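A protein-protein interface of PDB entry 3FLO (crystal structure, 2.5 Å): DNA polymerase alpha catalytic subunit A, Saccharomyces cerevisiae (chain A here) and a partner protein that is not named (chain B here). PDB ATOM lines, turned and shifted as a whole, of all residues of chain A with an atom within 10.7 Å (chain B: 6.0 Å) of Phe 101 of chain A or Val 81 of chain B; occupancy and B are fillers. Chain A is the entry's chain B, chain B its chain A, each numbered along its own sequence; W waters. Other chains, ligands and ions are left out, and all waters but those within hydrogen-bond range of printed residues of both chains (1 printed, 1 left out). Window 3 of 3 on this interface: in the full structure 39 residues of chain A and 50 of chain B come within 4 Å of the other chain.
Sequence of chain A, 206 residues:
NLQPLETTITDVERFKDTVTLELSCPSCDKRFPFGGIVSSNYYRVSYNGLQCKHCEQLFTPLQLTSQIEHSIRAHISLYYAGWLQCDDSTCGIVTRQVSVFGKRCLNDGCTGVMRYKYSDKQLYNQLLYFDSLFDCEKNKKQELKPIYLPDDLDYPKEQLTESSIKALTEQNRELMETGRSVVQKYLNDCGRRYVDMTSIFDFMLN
O of Val 98 of chain A touches OE2 of Glu 74 of chain B, 3.9 Å away. Ser 99 of chain A touches Ser 13 of chain B (O to CB, 3.5 Å). Glu 74 of chain B touches Ser 99 of chain A. Ser 13 of chain B touches Val 100 of chain A. Val 100 of chain A touches Thr 75 of chain B (CG2 to O, 3.4 Å). Gly 82 of chain B touches Val 100 of chain A (CA to CG2, 3.5 Å). Arg 77 of chain B touches Phe 101 of chain A (CG to CZ, 3.6 Å). Phe 101 of chain A touches Val 81 of chain B. Ser 13 of chain B touches Gly 102 of chain A. Arg 83 of chain B touches Arg 104 of chain A.
OE2 of Glu 74 of chain B lies within hydrogen-bond range of N of Val 100 of chain A. NE of Arg 77 of chain B is in hydrogen-bond range of O of Val 100 of chain A. The guanidinium group (NH2) of Arg 104 of chain A sits at hydrogen-bond distance from the backbone carbonyl oxygen (O) of Val 81 of chain B (2.9 Å). NH2 of Arg 104 of chain A sits close to O of Gly 82 of chain B, 3.4 Å away.
NH2 of Arg 77 of chain B sits at hydrogen-bond distance from OG of Ser 13 of chain B (3.1 Å). The guanidinium group (NH2) of Arg 83 of chain B lies within salt-bridge range of the side-chain carboxylate (OD2) of Asp 40 of chain B. The side-chain hydroxyl of Thr 75 of chain B sits close to the backbone carbonyl oxygen of Gly 80 of chain B. The backbone carbonyl oxygen of Arg 83 of chain B lies within hydrogen-bond range of the side-chain hydroxyl of Thr 75 of chain B, 2.9 Å away. N of Gly 82 of chain B sits at hydrogen-bond distance from O of Ser 76 of chain B. N of Phe 101 of chain A sits close to OG of Ser 99 of chain A (3.1 Å).
Water W1 lies within hydrogen-bond range of OE1 of Glu 74 of chain B and O of Val 98 of chain A.
Of the printed residues of chain B, Arg 104 of chain A touches Val 81 (2.9 Å), Gly 82 (3.3 Å) and Arg 83 (3.7 Å). Printed residues of chain A within 4 Å of Ser 13 of chain B: Ser 99 (3.5 Å), Val 100 (3.4 Å) and Gly 102 (3.4 Å). Ser 76 of chain B touches none of the printed residues of chain A. Printed residues of chain A within 4 Å of Arg 77 of chain B: Val 100 and Phe 101. No residue of chain A comes within 4 Å of Gly 79 of chain B. No residue of chain A comes within 4 Å of Gly 80 of chain B. Of the printed residues of chain A, Val 81 of chain B touches Phe 101 and Arg 104. The nearest printed residue of chain B that does not touch Phe 101 of chain A is Gly 82 of chain B (4.02 Å). The nearest residue of chain A that does not touch Val 81 of chain B is Val 100 of chain A (5.4 Å).
Of the 12 printed residues of chain B, 7 touch a printed residue of chain A. Printed residues of chain A that touch a printed residue of chain B: Val 98, Ser 99, Val 100, Phe 101, Gly 102 and Arg 104. Among the printed residues, no Asp or Glu carboxylate lies within 4 Å of a Lys or Arg side-chain nitrogen of the other chain.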
ATOM      1  N   LEU A  84      -3.907   6.343 -14.395  1.00  0.00           N
ATOM      2  CA  LEU A  84      -3.567   7.371 -13.427  1.00  0.00           C
ATOM      3  C   LEU A  84      -3.933   8.691 -14.023  1.00  0.00           C
ATOM      4  O   LEU A  84      -3.979   8.858 -15.245  1.00  0.00           O
ATOM      5  CB  LEU A  84      -2.073   7.345 -13.076  1.00  0.00           C
ATOM      6  CG  LEU A  84      -1.419   6.296 -12.154  1.00  0.00           C
ATOM      7  CD1 LEU A  84      -0.690   5.317 -12.920  1.00  0.00           C
ATOM      8  CD2 LEU A  84      -0.387   6.989 -11.211  1.00  0.00           C
ATOM      9  N   THR A  95      -2.722   8.336 -18.018  1.00  0.00           N
ATOM     10  CA  THR A  95      -1.699   7.463 -18.541  1.00  0.00           C
ATOM     11  C   THR A  95      -1.688   6.248 -17.659  1.00  0.00           C
ATOM     12  O   THR A  95      -2.199   6.281 -16.549  1.00  0.00           O
ATOM     13  CB  THR A  95      -0.341   8.170 -18.510  1.00  0.00           C
ATOM     14  OG1 THR A  95       0.681   7.292 -19.005  1.00  0.00           O
ATOM     15  CG2 THR A  95      -0.008   8.606 -17.099  1.00  0.00           C
ATOM     16  N   GLN A  97       1.429   4.819 -17.475  1.00  0.00           N
ATOM     17  CA  GLN A  97       2.854   4.879 -17.106  1.00  0.00           C
ATOM     18  C   GLN A  97       2.948   5.303 -15.639  1.00  0.00           C
ATOM     19  O   GLN A  97       2.209   6.204 -15.226  1.00  0.00           O
ATOM     20  CB  GLN A  97       3.570   5.925 -17.958  1.00  0.00           C
ATOM     21  CG  GLN A  97       3.865   5.534 -19.407  1.00  0.00           C
ATOM     22  CD  GLN A  97       4.813   4.367 -19.478  1.00  0.00           C
ATOM     23  OE1 GLN A  97       5.911   4.430 -18.938  1.00  0.00           O
ATOM     24  NE2 GLN A  97       4.385   3.277 -20.129  1.00  0.00           N
ATOM     25  N   VAL A  98       3.824   4.640 -14.865  1.00  0.00           N
ATOM     26  CA  VAL A  98       4.050   4.948 -13.457  1.00  0.00           C
ATOM     27  C   VAL A  98       5.532   5.270 -13.318  1.00  0.00           C
ATOM     28  O   VAL A  98       6.385   4.447 -13.633  1.00  0.00           O
ATOM     29  CB  VAL A  98       3.681   3.754 -12.548  1.00  0.00           C
ATOM     30  CG1 VAL A  98       3.965   4.066 -11.095  1.00  0.00           C
ATOM     31  CG2 VAL A  98       2.213   3.418 -12.673  1.00  0.00           C
ATOM     32  N   SER A  99       5.854   6.474 -12.868  1.00  0.00           N
ATOM     33  CA  SER A  99       7.222   6.789 -12.574  1.00  0.00           C
ATOM     34  C   SER A  99       7.673   6.071 -11.320  1.00  0.00           C
ATOM     35  O   SER A  99       6.890   5.862 -10.388  1.00  0.00           O
ATOM     36  CB  SER A  99       7.414   8.298 -12.422  1.00  0.00           C
ATOM     37  OG  SER A  99       8.719   8.596 -11.924  1.00  0.00           O
ATOM     38  N   VAL A 100       8.957   5.724 -11.293  1.00  0.00           N
ATOM     39  CA  VAL A 100       9.573   5.147 -10.124  1.00  0.00           C
ATOM     40  C   VAL A 100       9.415   6.055  -8.893  1.00  0.00           C
ATOM     41  O   VAL A 100       9.491   5.553  -7.793  1.00  0.00           O
ATOM     42  CB  VAL A 100      11.039   4.754 -10.443  1.00  0.00           C
ATOM     43  CG1 VAL A 100      11.050   3.676 -11.524  1.00  0.00           C
ATOM     44  CG2 VAL A 100      11.876   5.949 -10.849  1.00  0.00           C
ATOM     45  N   PHE A 101       9.161   7.356  -9.068  1.00  0.00           N
ATOM     46  CA  PHE A 101       8.493   8.197  -8.019  1.00  0.00           C
ATOM     47  C   PHE A 101       6.994   8.310  -8.381  1.00  0.00           C
ATOM     48  O   PHE A 101       6.589   9.171  -9.154  1.00  0.00           O
ATOM     49  CB  PHE A 101       9.101   9.581  -7.944  1.00  0.00           C
ATOM     50  CG  PHE A 101      10.506   9.615  -7.397  1.00  0.00           C
ATOM     51  CD1 PHE A 101      10.740   9.506  -6.039  1.00  0.00           C
ATOM     52  CD2 PHE A 101      11.593   9.814  -8.244  1.00  0.00           C
ATOM     53  CE1 PHE A 101      12.037   9.571  -5.526  1.00  0.00           C
ATOM     54  CE2 PHE A 101      12.909   9.893  -7.740  1.00  0.00           C
ATOM     55  CZ  PHE A 101      13.125   9.772  -6.375  1.00  0.00           C
ATOM     56  N   GLY A 102       6.183   7.429  -7.800  1.00  0.00           N
ATOM     57  CA  GLY A 102       4.792   7.199  -8.230  1.00  0.00           C
ATOM     58  C   GLY A 102       3.928   8.426  -8.395  1.00  0.00           C
ATOM     59  O   GLY A 102       3.238   8.562  -9.390  1.00  0.00           O
ATOM     60  N   LYS A 103       4.003   9.324  -7.424  1.00  0.00           N
ATOM     61  CA  LYS A 103       3.126  10.487  -7.359  1.00  0.00           C
ATOM     62  C   LYS A 103       3.533  11.565  -8.352  1.00  0.00           C
ATOM     63  O   LYS A 103       2.770  12.496  -8.606  1.00  0.00           O
ATOM     64  CB  LYS A 103       3.119  11.039  -5.906  1.00  0.00           C
ATOM     65  CG  LYS A 103       2.340  10.096  -4.921  1.00  0.00           C
ATOM     66  CD  LYS A 103       2.111  10.692  -3.506  1.00  0.00           C
ATOM     67  CE  LYS A 103       1.133   9.771  -2.715  1.00  0.00           C
ATOM     68  NZ  LYS A 103       0.376  10.415  -1.511  1.00  0.00           N
ATOM     69  N   ARG A 104       4.725  11.426  -8.921  1.00  0.00           N
ATOM     70  CA  ARG A 104       5.281  12.451  -9.802  1.00  0.00           C
ATOM     71  C   ARG A 104       4.737  12.371 -11.225  1.00  0.00           C
ATOM     72  O   ARG A 104       4.667  11.301 -11.817  1.00  0.00           O
ATOM     73  CB  ARG A 104       6.785  12.340  -9.864  1.00  0.00           C
ATOM     74  CG  ARG A 104       7.367  13.420 -10.713  1.00  0.00           C
ATOM     75  CD  ARG A 104       8.833  13.603 -10.480  1.00  0.00           C
ATOM     76  NE  ARG A 104       9.609  12.583 -11.179  1.00  0.00           N
ATOM     77  CZ  ARG A 104      10.921  12.423 -11.041  1.00  0.00           C
ATOM     78  NH1 ARG A 104      11.606  13.201 -10.215  1.00  0.00           N
ATOM     79  NH2 ARG A 104      11.553  11.477 -11.720  1.00  0.00           N
ATOM     80  N   CYS A 105       4.362  13.519 -11.763  1.00  0.00           N
ATOM     81  CA  CYS A 105       3.788  13.608 -13.102  1.00  0.00           C
ATOM     82  C   CYS A 105       4.852  13.501 -14.165  1.00  0.00           C
ATOM     83  O   CYS A 105       5.909  14.064 -14.032  1.00  0.00           O
ATOM     84  CB  CYS A 105       3.095  14.957 -13.272  1.00  0.00           C
ATOM     85  SG  CYS A 105       2.098  15.085 -14.766  1.00  0.00           S
ATOM     86  N   LEU A 106       4.554  12.786 -15.234  1.00  0.00           N
ATOM     87  CA  LEU A 106       5.522  12.562 -16.308  1.00  0.00           C
ATOM     88  C   LEU A 106       5.642  13.696 -17.329  1.00  0.00           C
ATOM     89  O   LEU A 106       6.561  13.646 -18.144  1.00  0.00           O
ATOM     90  CB  LEU A 106       5.234  11.253 -17.035  1.00  0.00           C
ATOM     91  CG  LEU A 106       5.597  10.040 -16.208  1.00  0.00           C
ATOM     92  CD1 LEU A 106       5.068   8.796 -16.866  1.00  0.00           C
ATOM     93  CD2 LEU A 106       7.071   9.990 -16.008  1.00  0.00           C
ATOM     94  N   ASN A 107       4.769  14.712 -17.287  1.00  0.00           N
ATOM     95  CA  ASN A 107       4.983  15.968 -18.087  1.00  0.00           C
ATOM     96  C   ASN A 107       6.170  16.806 -17.631  1.00  0.00           C
ATOM     97  O   ASN A 107       6.174  17.324 -16.507  1.00  0.00           O
ATOM     98  CB  ASN A 107       3.831  16.966 -17.998  1.00  0.00           C
ATOM     99  CG  ASN A 107       2.816  16.780 -19.073  1.00  0.00           C
ATOM    100  OD1 ASN A 107       2.573  15.660 -19.504  1.00  0.00           O
ATOM    101  ND2 ASN A 107       2.177  17.873 -19.494  1.00  0.00           N
ATOM    102  N   ASP A 108       7.138  17.013 -18.508  1.00  0.00           N
ATOM    103  CA  ASP A 108       8.277  17.820 -18.130  1.00  0.00           C
ATOM    104  C   ASP A 108       7.832  18.970 -17.211  1.00  0.00           C
ATOM    105  O   ASP A 108       7.092  19.870 -17.626  1.00  0.00           O
ATOM    106  CB  ASP A 108       9.009  18.384 -19.365  1.00  0.00           C
ATOM    107  CG  ASP A 108      10.515  18.392 -19.176  1.00  0.00           C
ATOM    108  OD1 ASP A 108      11.029  17.329 -18.738  1.00  0.00           O
ATOM    109  OD2 ASP A 108      11.176  19.443 -19.438  1.00  0.00           O
ATOM    110  N   CYS A 110       5.904  19.402 -14.623  1.00  0.00           N
ATOM    111  CA  CYS A 110       4.587  19.565 -14.049  1.00  0.00           C
ATOM    112  C   CYS A 110       4.642  19.183 -12.566  1.00  0.00           C
ATOM    113  O   CYS A 110       5.233  18.164 -12.209  1.00  0.00           O
ATOM    114  CB  CYS A 110       3.587  18.694 -14.785  1.00  0.00           C
ATOM    115  SG  CYS A 110       2.005  18.696 -13.998  1.00  0.00           S
ATOM    116  N   THR A 111       4.043  19.992 -11.698  1.00  0.00           N
ATOM    117  CA  THR A 111       4.168  19.777 -10.245  1.00  0.00           C
ATOM    118  C   THR A 111       2.945  19.101  -9.629  1.00  0.00           C
ATOM    119  O   THR A 111       2.848  18.983  -8.407  1.00  0.00           O
ATOM    120  CB  THR A 111       4.423  21.078  -9.517  1.00  0.00           C
ATOM    121  OG1 THR A 111       3.294  21.928  -9.701  1.00  0.00           O
ATOM    122  CG2 THR A 111       5.656  21.749 -10.059  1.00  0.00           C
ATOM    123  N   GLY A 112       2.024  18.647 -10.468  1.00  0.00           N
ATOM    124  CA  GLY A 112       0.815  18.024  -9.993  1.00  0.00           C
ATOM    125  C   GLY A 112       1.075  16.646  -9.424  1.00  0.00           C
ATOM    126  O   GLY A 112       2.133  16.063  -9.629  1.00  0.00           O
ATOM    127  N   VAL A 113       0.103  16.127  -8.692  1.00  0.00           N
ATOM    128  CA  VAL A 113       0.224  14.818  -8.076  1.00  0.00           C
ATOM    129  C   VAL A 113      -0.595  13.786  -8.860  1.00  0.00           C
ATOM    130  O   VAL A 113      -1.667  14.067  -9.315  1.00  0.00           O
ATOM    131  CB  VAL A 113      -0.231  14.867  -6.614  1.00  0.00           C
ATOM    132  CG1 VAL A 113      -0.210  13.454  -5.998  1.00  0.00           C
ATOM    133  CG2 VAL A 113       0.627  15.847  -5.837  1.00  0.00           C
ATOM    134  N   MET A 114      -0.051  12.603  -9.046  1.00  0.00           N
ATOM    135  CA  MET A 114      -0.697  11.567  -9.802  1.00  0.00           C
ATOM    136  C   MET A 114      -1.491  10.690  -8.853  1.00  0.00           C
ATOM    137  O   MET A 114      -1.047  10.416  -7.737  1.00  0.00           O
ATOM    138  CB  MET A 114       0.350  10.716 -10.514  1.00  0.00           C
ATOM    139  CG  MET A 114       1.110  11.362 -11.656  1.00  0.00           C
ATOM    140  SD  MET A 114       0.107  12.102 -12.969  1.00  0.00           S
ATOM    141  CE  MET A 114      -0.799  10.733 -13.741  1.00  0.00           C
ATOM    142  N   ARG A 115      -2.687  10.288  -9.284  1.00  0.00           N
ATOM    143  CA  ARG A 115      -3.559   9.419  -8.493  1.00  0.00           C
ATOM    144  C   ARG A 115      -4.211   8.413  -9.396  1.00  0.00           C
ATOM    145  O   ARG A 115      -4.574   8.748 -10.524  1.00  0.00           O
ATOM    146  CB  ARG A 115      -4.658  10.214  -7.829  1.00  0.00           C
ATOM    147  CG  ARG A 115      -4.159  11.156  -6.766  1.00  0.00           C
ATOM    148  CD  ARG A 115      -5.309  11.942  -6.090  1.00  0.00           C
ATOM    149  NE  ARG A 115      -4.876  13.314  -5.796  1.00  0.00           N
ATOM    150  CZ  ARG A 115      -3.999  13.642  -4.858  1.00  0.00           C
ATOM    151  NH1 ARG A 115      -3.441  12.700  -4.101  1.00  0.00           N
ATOM    152  NH2 ARG A 115      -3.670  14.917  -4.670  1.00  0.00           N
ATOM    153  N   TYR A 116      -4.346   7.185  -8.906  1.00  0.00           N
ATOM    154  CA  TYR A 116      -5.087   6.167  -9.604  1.00  0.00           C
ATOM    155  C   TYR A 116      -6.466   6.725  -9.928  1.00  0.00           C
ATOM    156  O   TYR A 116      -7.138   7.191  -9.047  1.00  0.00           O
ATOM    157  CB  TYR A 116      -5.178   4.908  -8.730  1.00  0.00           C
ATOM    158  CG  TYR A 116      -3.965   4.001  -8.806  1.00  0.00           C
ATOM    159  CD1 TYR A 116      -3.558   3.487 -10.011  1.00  0.00           C
ATOM    160  CD2 TYR A 116      -3.237   3.648  -7.675  1.00  0.00           C
ATOM    161  CE1 TYR A 116      -2.450   2.671 -10.120  1.00  0.00           C
ATOM    162  CE2 TYR A 116      -2.128   2.794  -7.770  1.00  0.00           C
ATOM    163  CZ  TYR A 116      -1.746   2.317  -9.008  1.00  0.00           C
ATOM    164  OH  TYR A 116      -0.657   1.464  -9.189  1.00  0.00           O
ATOM    165  N   SER B  13       5.344   1.869  -7.227  1.00  0.00           N
ATOM    166  CA  SER B  13       6.515   2.508  -7.698  1.00  0.00           C
ATOM    167  C   SER B  13       7.761   1.878  -7.040  1.00  0.00           C
ATOM    168  O   SER B  13       8.758   1.679  -7.713  1.00  0.00           O
ATOM    169  CB  SER B  13       6.465   4.026  -7.466  1.00  0.00           C
ATOM    170  OG  SER B  13       6.440   4.303  -6.065  1.00  0.00           O
ATOM    171  N   ASP B  40      24.471   8.538 -14.557  1.00  0.00           N
ATOM    172  CA  ASP B  40      23.166   9.000 -14.887  1.00  0.00           C
ATOM    173  C   ASP B  40      23.126   9.341 -16.382  1.00  0.00           C
ATOM    174  O   ASP B  40      23.703  10.331 -16.799  1.00  0.00           O
ATOM    175  CB  ASP B  40      22.885  10.241 -14.054  1.00  0.00           C
ATOM    176  CG  ASP B  40      21.525  10.840 -14.322  1.00  0.00           C
ATOM    177  OD1 ASP B  40      20.799  10.401 -15.264  1.00  0.00           O
ATOM    178  OD2 ASP B  40      21.196  11.768 -13.556  1.00  0.00           O
ATOM    179  N   GLU B  74      14.002   4.810 -18.637  1.00  0.00           N
ATOM    180  CA  GLU B  74      13.723   5.307 -17.307  1.00  0.00           C
ATOM    181  C   GLU B  74      14.791   4.813 -16.370  1.00  0.00           C
ATOM    182  O   GLU B  74      15.071   3.609 -16.337  1.00  0.00           O
ATOM    183  CB  GLU B  74      12.359   4.798 -16.804  1.00  0.00           C
ATOM    184  CG  GLU B  74      12.069   5.254 -15.404  1.00  0.00           C
ATOM    185  CD  GLU B  74      10.745   4.723 -14.895  1.00  0.00           C
ATOM    186  OE1 GLU B  74      10.422   3.515 -15.097  1.00  0.00           O
ATOM    187  OE2 GLU B  74      10.037   5.528 -14.248  1.00  0.00           O
ATOM    188  N   THR B  75      15.342   5.727 -15.573  1.00  0.00           N
ATOM    189  CA  THR B  75      16.331   5.395 -14.558  1.00  0.00           C
ATOM    190  C   THR B  75      15.688   5.135 -13.155  1.00  0.00           C
ATOM    191  O   THR B  75      14.552   5.566 -12.872  1.00  0.00           O
ATOM    192  CB  THR B  75      17.341   6.547 -14.414  1.00  0.00           C
ATOM    193  OG1 THR B  75      16.661   7.737 -13.944  1.00  0.00           O
ATOM    194  CG2 THR B  75      18.057   6.829 -15.755  1.00  0.00           C
ATOM    195  N   SER B  76      16.425   4.448 -12.289  1.00  0.00           N
ATOM    196  CA  SER B  76      15.998   4.224 -10.921  1.00  0.00           C
ATOM    197  C   SER B  76      16.091   5.521 -10.163  1.00  0.00           C
ATOM    198  O   SER B  76      16.639   6.528 -10.676  1.00  0.00           O
ATOM    199  CB  SER B  76      16.889   3.204 -10.253  1.00  0.00           C
ATOM    200  OG  SER B  76      18.150   3.789  -9.933  1.00  0.00           O
ATOM    201  N   ARG B  77      15.581   5.494  -8.929  1.00  0.00           N
ATOM    202  CA  ARG B  77      15.567   6.679  -8.108  1.00  0.00           C
ATOM    203  C   ARG B  77      16.987   7.109  -7.746  1.00  0.00           C
ATOM    204  O   ARG B  77      17.249   8.288  -7.667  1.00  0.00           O
ATOM    205  CB  ARG B  77      14.800   6.460  -6.829  1.00  0.00           C
ATOM    206  CG  ARG B  77      13.359   6.226  -6.991  1.00  0.00           C
ATOM    207  CD  ARG B  77      12.764   5.730  -5.662  1.00  0.00           C
ATOM    208  NE  ARG B  77      11.432   5.216  -5.923  1.00  0.00           N
ATOM    209  CZ  ARG B  77      10.681   4.581  -5.054  1.00  0.00           C
ATOM    210  NH1 ARG B  77      11.128   4.339  -3.842  1.00  0.00           N
ATOM    211  NH2 ARG B  77       9.464   4.189  -5.398  1.00  0.00           N
ATOM    212  N   MET B  78      17.874   6.149  -7.480  1.00  0.00           N
ATOM    213  CA  MET B  78      19.265   6.463  -7.159  1.00  0.00           C
ATOM    214  C   MET B  78      20.097   6.760  -8.414  1.00  0.00           C
ATOM    215  O   MET B  78      20.996   7.573  -8.390  1.00  0.00           O
ATOM    216  CB  MET B  78      19.922   5.309  -6.431  1.00  0.00           C
ATOM    217  CG  MET B  78      19.342   5.065  -5.073  1.00  0.00           C
ATOM    218  SD  MET B  78      20.471   4.124  -4.019  1.00  0.00           S
ATOM    219  CE  MET B  78      22.085   4.951  -4.285  1.00  0.00           C
ATOM    220  N   GLY B  79      19.778   6.076  -9.502  1.00  0.00           N
ATOM    221  CA  GLY B  79      20.535   6.184 -10.736  1.00  0.00           C
ATOM    222  C   GLY B  79      20.418   7.532 -11.401  1.00  0.00           C
ATOM    223  O   GLY B  79      21.418   8.117 -11.756  1.00  0.00           O
ATOM    224  N   GLY B  80      19.201   8.039 -11.559  1.00  0.00           N
ATOM    225  CA  GLY B  80      18.979   9.340 -12.215  1.00  0.00           C
ATOM    226  C   GLY B  80      17.772  10.106 -11.690  1.00  0.00           C
ATOM    227  O   GLY B  80      17.077  10.784 -12.455  1.00  0.00           O
ATOM    228  N   VAL B  81      17.508   9.978 -10.387  1.00  0.00           N
ATOM    229  CA  VAL B  81      16.377  10.625  -9.742  1.00  0.00           C
ATOM    230  C   VAL B  81      15.104  10.283 -10.524  1.00  0.00           C
ATOM    231  O   VAL B  81      14.193  11.104 -10.658  1.00  0.00           O
ATOM    232  CB  VAL B  81      16.577  12.204  -9.648  1.00  0.00           C
ATOM    233  CG1 VAL B  81      15.810  12.813  -8.483  1.00  0.00           C
ATOM    234  CG2 VAL B  81      18.060  12.598  -9.520  1.00  0.00           C
ATOM    235  N   GLY B  82      15.044   9.065 -11.039  1.00  0.00           N
ATOM    236  CA  GLY B  82      13.902   8.608 -11.756  1.00  0.00           C
ATOM    237  C   GLY B  82      13.618   9.260 -13.078  1.00  0.00           C
ATOM    238  O   GLY B  82      12.620   8.946 -13.710  1.00  0.00           O
ATOM    239  N   ARG B  83      14.503  10.132 -13.534  1.00  0.00           N
ATOM    240  CA  ARG B  83      14.291  10.800 -14.834  1.00  0.00           C
ATOM    241  C   ARG B  83      14.298   9.829 -16.011  1.00  0.00           C
ATOM    242  O   ARG B  83      14.902   8.743 -15.951  1.00  0.00           O
ATOM    243  CB  ARG B  83      15.331  11.889 -15.084  1.00  0.00           C
ATOM    244  CG  ARG B  83      15.094  13.181 -14.263  1.00  0.00           C
ATOM    245  CD  ARG B  83      16.095  14.283 -14.621  1.00  0.00           C
ATOM    246  NE  ARG B  83      17.469  13.786 -14.425  1.00  0.00           N
ATOM    247  CZ  ARG B  83      18.220  14.011 -13.343  1.00  0.00           C
ATOM    248  NH1 ARG B  83      17.812  14.800 -12.358  1.00  0.00           N
ATOM    249  NH2 ARG B  83      19.415  13.468 -13.260  1.00  0.00           N
HETATM  250  O   HOH W   1       8.048   2.609 -14.795  1.00  0.00           O
